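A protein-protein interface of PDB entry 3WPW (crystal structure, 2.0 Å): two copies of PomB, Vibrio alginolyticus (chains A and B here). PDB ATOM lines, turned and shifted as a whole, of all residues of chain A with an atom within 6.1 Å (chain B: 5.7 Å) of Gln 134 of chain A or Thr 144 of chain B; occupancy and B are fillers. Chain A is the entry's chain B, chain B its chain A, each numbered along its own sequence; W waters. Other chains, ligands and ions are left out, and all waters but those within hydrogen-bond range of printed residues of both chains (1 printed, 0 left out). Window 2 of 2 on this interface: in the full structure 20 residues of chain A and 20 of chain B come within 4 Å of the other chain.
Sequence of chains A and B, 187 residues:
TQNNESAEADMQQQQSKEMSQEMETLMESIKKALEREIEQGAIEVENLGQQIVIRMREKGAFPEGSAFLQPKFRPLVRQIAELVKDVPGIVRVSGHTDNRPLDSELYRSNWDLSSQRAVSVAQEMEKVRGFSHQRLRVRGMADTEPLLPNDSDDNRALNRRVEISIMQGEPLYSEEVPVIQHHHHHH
O of Thr 144 of chain B sits at hydrogen-bond distance from NE2 of Gln 134 of chain A, at 2.8 Å. OD1 of Asp 143 of chain B is in hydrogen-bond range of NE2 of His 133 of chain A.
The backbone carbonyl oxygen of Met 141 of chain B lies within hydrogen-bond range of the side-chain hydroxyl of Thr 144 of chain B, 2.7 Å away. OG of Ser 132 of chain A lies close to N of Gln 134 of chain A, 3.4 Å away. NH1 of Arg 137 of chain A sits at hydrogen-bond distance from O of Gln 134 of chain A, 2.8 Å away.
Among the printed residues, pairs that only touch across the chains: Leu 136 of chain A with Trp 111 of chain B (3.2 Å), Arg 137 of chain A with Met 141 of chain B (3.3 Å), Arg 137 of chain A with Thr 144 of chain B (3.5 Å), His 133 of chain A with Trp 111 of chain B (3.5 Å) and Leu 136 of chain A with Thr 144 of chain B (3.7 Å).
Gln 134 of chain A touches one residue of chain B. Of the printed residues of chain A, Met 141 of chain B touches Arg 137. Printed residues of chain A within 4 Å of Asp 143 of chain B: His 133. Thr 144 of chain B touches three residues of chain A. The nearest residue of chain B that does not touch Gln 134 of chain A is Asp 143 of chain B (4.4 Å). The nearest residue of chain A that does not touch Thr 144 of chain B is His 133 of chain A (4.1 Å). The nearest printed residue of chain B that does not touch Leu 136 of chain A is Met 141 of chain B (5.4 Å).
Hydrophobic or aromatic side chains of chain A that line the printed part of chain B: His 133 and Leu 136. Among the printed residues, no Asp or Glu carboxylate lies within 4 Å of a Lys or Arg side-chain nitrogen of the other chain.
No position is printed for both chains.
Water W1 bridges the guanidinium group (NE) of Arg 137 of chain A (3.2 Å) and the side-chain carboxylate (OE1) of Glu 145 of chain B (3.5 Å).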
ATOM      1  N   ILE A  90     -19.232  -7.388 -21.499  1.00  0.00           N
ATOM      2  CA  ILE A  90     -18.983  -6.697 -20.240  1.00  0.00           C
ATOM      3  C   ILE A  90     -20.167  -5.800 -19.864  1.00  0.00           C
ATOM      4  O   ILE A  90     -20.797  -5.190 -20.726  1.00  0.00           O
ATOM      5  CB  ILE A  90     -17.711  -5.830 -20.326  1.00  0.00           C
ATOM      6  CG1 ILE A  90     -16.475  -6.713 -20.464  1.00  0.00           C
ATOM      7  CG2 ILE A  90     -17.568  -4.973 -19.076  1.00  0.00           C
ATOM      8  CD1 ILE A  90     -16.232  -7.589 -19.249  1.00  0.00           C
ATOM      9  N   SER A 132     -23.855 -13.168 -14.455  1.00  0.00           N
ATOM     10  CA  SER A 132     -22.441 -13.462 -14.199  1.00  0.00           C
ATOM     11  C   SER A 132     -21.624 -12.307 -13.572  1.00  0.00           C
ATOM     12  O   SER A 132     -21.445 -11.238 -14.174  1.00  0.00           O
ATOM     13  CB  SER A 132     -21.765 -13.929 -15.490  1.00  0.00           C
ATOM     14  OG  SER A 132     -20.382 -14.190 -15.278  1.00  0.00           O
ATOM     15  N   HIS A 133     -21.132 -12.560 -12.364  1.00  0.00           N
ATOM     16  CA  HIS A 133     -20.232 -11.668 -11.621  1.00  0.00           C
ATOM     17  C   HIS A 133     -19.030 -11.254 -12.465  1.00  0.00           C
ATOM     18  O   HIS A 133     -18.591 -10.106 -12.415  1.00  0.00           O
ATOM     19  CB  HIS A 133     -19.792 -12.390 -10.326  1.00  0.00           C
ATOM     20  CG  HIS A 133     -18.546 -11.845  -9.685  1.00  0.00           C
ATOM     21  ND1 HIS A 133     -18.568 -10.834  -8.743  1.00  0.00           N
ATOM     22  CD2 HIS A 133     -17.247 -12.217  -9.797  1.00  0.00           C
ATOM     23  CE1 HIS A 133     -17.339 -10.594  -8.323  1.00  0.00           C
ATOM     24  NE2 HIS A 133     -16.517 -11.425  -8.943  1.00  0.00           N
ATOM     25  N   GLN A 134     -18.512 -12.199 -13.249  1.00  0.00           N
ATOM     26  CA  GLN A 134     -17.291 -12.005 -14.027  1.00  0.00           C
ATOM     27  C   GLN A 134     -17.405 -10.922 -15.091  1.00  0.00           C
ATOM     28  O   GLN A 134     -16.395 -10.391 -15.561  1.00  0.00           O
ATOM     29  CB  GLN A 134     -16.894 -13.318 -14.708  1.00  0.00           C
ATOM     30  CG  GLN A 134     -15.704 -13.203 -15.665  1.00  0.00           C
ATOM     31  CD  GLN A 134     -14.381 -12.839 -14.957  1.00  0.00           C
ATOM     32  OE1 GLN A 134     -14.161 -13.194 -13.791  1.00  0.00           O
ATOM     33  NE2 GLN A 134     -13.497 -12.133 -15.673  1.00  0.00           N
ATOM     34  N   ARG A 135     -18.622 -10.602 -15.501  1.00  0.00           N
ATOM     35  CA  ARG A 135     -18.767  -9.623 -16.570  1.00  0.00           C
ATOM     36  C   ARG A 135     -18.811  -8.162 -16.093  1.00  0.00           C
ATOM     37  O   ARG A 135     -18.783  -7.244 -16.907  1.00  0.00           O
ATOM     38  CB  ARG A 135     -19.956  -9.968 -17.485  1.00  0.00           C
ATOM     39  CG  ARG A 135     -21.311  -9.860 -16.863  1.00  0.00           C
ATOM     40  CD  ARG A 135     -22.364 -10.556 -17.774  1.00  0.00           C
ATOM     41  NE  ARG A 135     -22.695  -9.773 -18.967  1.00  0.00           N
ATOM     42  CZ  ARG A 135     -23.899  -9.759 -19.533  1.00  0.00           C
ATOM     43  NH1 ARG A 135     -24.880 -10.504 -19.027  1.00  0.00           N
ATOM     44  NH2 ARG A 135     -24.128  -9.010 -20.602  1.00  0.00           N
ATOM     45  N   LEU A 136     -18.867  -7.957 -14.782  1.00  0.00           N
ATOM     46  CA  LEU A 136     -19.054  -6.618 -14.235  1.00  0.00           C
ATOM     47  C   LEU A 136     -17.721  -5.879 -14.153  1.00  0.00           C
ATOM     48  O   LEU A 136     -16.668  -6.499 -14.020  1.00  0.00           O
ATOM     49  CB  LEU A 136     -19.658  -6.698 -12.834  1.00  0.00           C
ATOM     50  CG  LEU A 136     -21.170  -6.855 -12.709  1.00  0.00           C
ATOM     51  CD1 LEU A 136     -21.550  -7.377 -11.335  1.00  0.00           C
ATOM     52  CD2 LEU A 136     -21.853  -5.523 -13.008  1.00  0.00           C
ATOM     53  N   ARG A 137     -17.789  -4.555 -14.228  1.00  0.00           N
ATOM     54  CA  ARG A 137     -16.652  -3.684 -13.964  1.00  0.00           C
ATOM     55  C   ARG A 137     -17.244  -2.434 -13.314  1.00  0.00           C
ATOM     56  O   ARG A 137     -18.231  -1.908 -13.814  1.00  0.00           O
ATOM     57  CB  ARG A 137     -15.949  -3.291 -15.278  1.00  0.00           C
ATOM     58  CG  ARG A 137     -15.393  -4.448 -16.112  1.00  0.00           C
ATOM     59  CD  ARG A 137     -14.330  -5.220 -15.346  1.00  0.00           C
ATOM     60  NE  ARG A 137     -13.621  -6.175 -16.196  1.00  0.00           N
ATOM     61  CZ  ARG A 137     -14.047  -7.411 -16.456  1.00  0.00           C
ATOM     62  NH1 ARG A 137     -15.199  -7.839 -15.956  1.00  0.00           N
ATOM     63  NH2 ARG A 137     -13.331  -8.213 -17.238  1.00  0.00           N
ATOM     64  N   THR B  97      -8.681  -7.576  -6.475  1.00  0.00           N
ATOM     65  CA  THR B  97      -8.610  -8.480  -5.331  1.00  0.00           C
ATOM     66  C   THR B  97      -8.341  -9.893  -5.848  1.00  0.00           C
ATOM     67  O   THR B  97      -8.381 -10.141  -7.067  1.00  0.00           O
ATOM     68  CB  THR B  97      -9.939  -8.518  -4.526  1.00  0.00           C
ATOM     69  OG1 THR B  97     -10.980  -9.040  -5.354  1.00  0.00           O
ATOM     70  CG2 THR B  97     -10.334  -7.134  -4.031  1.00  0.00           C
ATOM     71  N   TRP B 111     -15.778  -5.609  -4.828  1.00  0.00           N
ATOM     72  CA  TRP B 111     -15.975  -4.413  -5.673  1.00  0.00           C
ATOM     73  C   TRP B 111     -15.700  -3.155  -4.871  1.00  0.00           C
ATOM     74  O   TRP B 111     -15.069  -2.184  -5.340  1.00  0.00           O
ATOM     75  CB  TRP B 111     -17.411  -4.333  -6.213  1.00  0.00           C
ATOM     76  CG  TRP B 111     -17.814  -5.480  -7.104  1.00  0.00           C
ATOM     77  CD1 TRP B 111     -18.782  -6.428  -6.844  1.00  0.00           C
ATOM     78  CD2 TRP B 111     -17.277  -5.799  -8.386  1.00  0.00           C
ATOM     79  NE1 TRP B 111     -18.868  -7.312  -7.895  1.00  0.00           N
ATOM     80  CE2 TRP B 111     -17.958  -6.948  -8.857  1.00  0.00           C
ATOM     81  CE3 TRP B 111     -16.289  -5.228  -9.194  1.00  0.00           C
ATOM     82  CZ2 TRP B 111     -17.667  -7.536 -10.085  1.00  0.00           C
ATOM     83  CZ3 TRP B 111     -16.003  -5.820 -10.419  1.00  0.00           C
ATOM     84  CH2 TRP B 111     -16.686  -6.960 -10.849  1.00  0.00           C
ATOM     85  N   MET B 141     -12.048  -3.698 -10.009  1.00  0.00           N
ATOM     86  CA  MET B 141     -12.099  -4.854 -10.891  1.00  0.00           C
ATOM     87  C   MET B 141     -12.378  -6.124 -10.108  1.00  0.00           C
ATOM     88  O   MET B 141     -12.478  -7.201 -10.681  1.00  0.00           O
ATOM     89  CB  MET B 141     -10.762  -5.013 -11.595  1.00  0.00           C
ATOM     90  CG  MET B 141     -10.293  -3.784 -12.357  1.00  0.00           C
ATOM     91  SD  MET B 141     -11.360  -3.382 -13.746  1.00  0.00           S
ATOM     92  CE  MET B 141     -10.994  -4.749 -14.848  1.00  0.00           C
ATOM     93  N   ALA B 142     -12.457  -5.996  -8.791  1.00  0.00           N
ATOM     94  CA  ALA B 142     -12.602  -7.161  -7.927  1.00  0.00           C
ATOM     95  C   ALA B 142     -11.654  -8.251  -8.417  1.00  0.00           C
ATOM     96  O   ALA B 142     -10.455  -7.997  -8.637  1.00  0.00           O
ATOM     97  CB  ALA B 142     -14.038  -7.634  -7.918  1.00  0.00           C
ATOM     98  N   ASP B 143     -12.186  -9.453  -8.614  1.00  0.00           N
ATOM     99  CA  ASP B 143     -11.365 -10.590  -9.008  1.00  0.00           C
ATOM    100  C   ASP B 143     -11.479 -10.915 -10.484  1.00  0.00           C
ATOM    101  O   ASP B 143     -11.068 -11.988 -10.919  1.00  0.00           O
ATOM    102  CB  ASP B 143     -11.739 -11.836  -8.179  1.00  0.00           C
ATOM    103  CG  ASP B 143     -13.193 -12.234  -8.323  1.00  0.00           C
ATOM    104  OD1 ASP B 143     -14.022 -11.364  -8.657  1.00  0.00           O
ATOM    105  OD2 ASP B 143     -13.516 -13.425  -8.091  1.00  0.00           O
ATOM    106  N   THR B 144     -12.014  -9.988 -11.266  1.00  0.00           N
ATOM    107  CA  THR B 144     -12.314 -10.293 -12.664  1.00  0.00           C
ATOM    108  C   THR B 144     -11.098 -10.362 -13.585  1.00  0.00           C
ATOM    109  O   THR B 144     -11.194 -10.881 -14.696  1.00  0.00           O
ATOM    110  CB  THR B 144     -13.290  -9.276 -13.281  1.00  0.00           C
ATOM    111  OG1 THR B 144     -12.656  -7.994 -13.308  1.00  0.00           O
ATOM    112  CG2 THR B 144     -14.605  -9.212 -12.488  1.00  0.00           C
ATOM    113  N   GLU B 145      -9.970  -9.803 -13.163  1.00  0.00           N
ATOM    114  CA  GLU B 145      -8.772  -9.844 -14.003  1.00  0.00           C
ATOM    115  C   GLU B 145      -7.557 -10.364 -13.240  1.00  0.00           C
ATOM    116  O   GLU B 145      -6.627  -9.591 -12.938  1.00  0.00           O
ATOM    117  CB  GLU B 145      -8.421  -8.447 -14.551  1.00  0.00           C
ATOM    118  CG  GLU B 145      -9.418  -7.883 -15.530  1.00  0.00           C
ATOM    119  CD  GLU B 145      -8.869  -6.668 -16.260  1.00  0.00           C
ATOM    120  OE1 GLU B 145      -9.346  -6.410 -17.381  1.00  0.00           O
ATOM    121  OE2 GLU B 145      -7.960  -5.979 -15.717  1.00  0.00           O
ATOM    122  N   PRO B 146      -7.551 -11.668 -12.917  1.00  0.00           N
ATOM    123  CA  PRO B 146      -6.379 -12.201 -12.223  1.00  0.00           C
ATOM    124  C   PRO B 146      -5.104 -12.093 -13.062  1.00  0.00           C
ATOM    125  O   PRO B 146      -5.146 -12.199 -14.290  1.00  0.00           O
ATOM    126  CB  PRO B 146      -6.746 -13.681 -11.988  1.00  0.00           C
ATOM    127  CG  PRO B 146      -7.860 -13.985 -12.948  1.00  0.00           C
ATOM    128  CD  PRO B 146      -8.609 -12.678 -13.105  1.00  0.00           C
HETATM  129  O   HOH W   1     -12.222  -5.217 -18.872  1.00  0.00           O
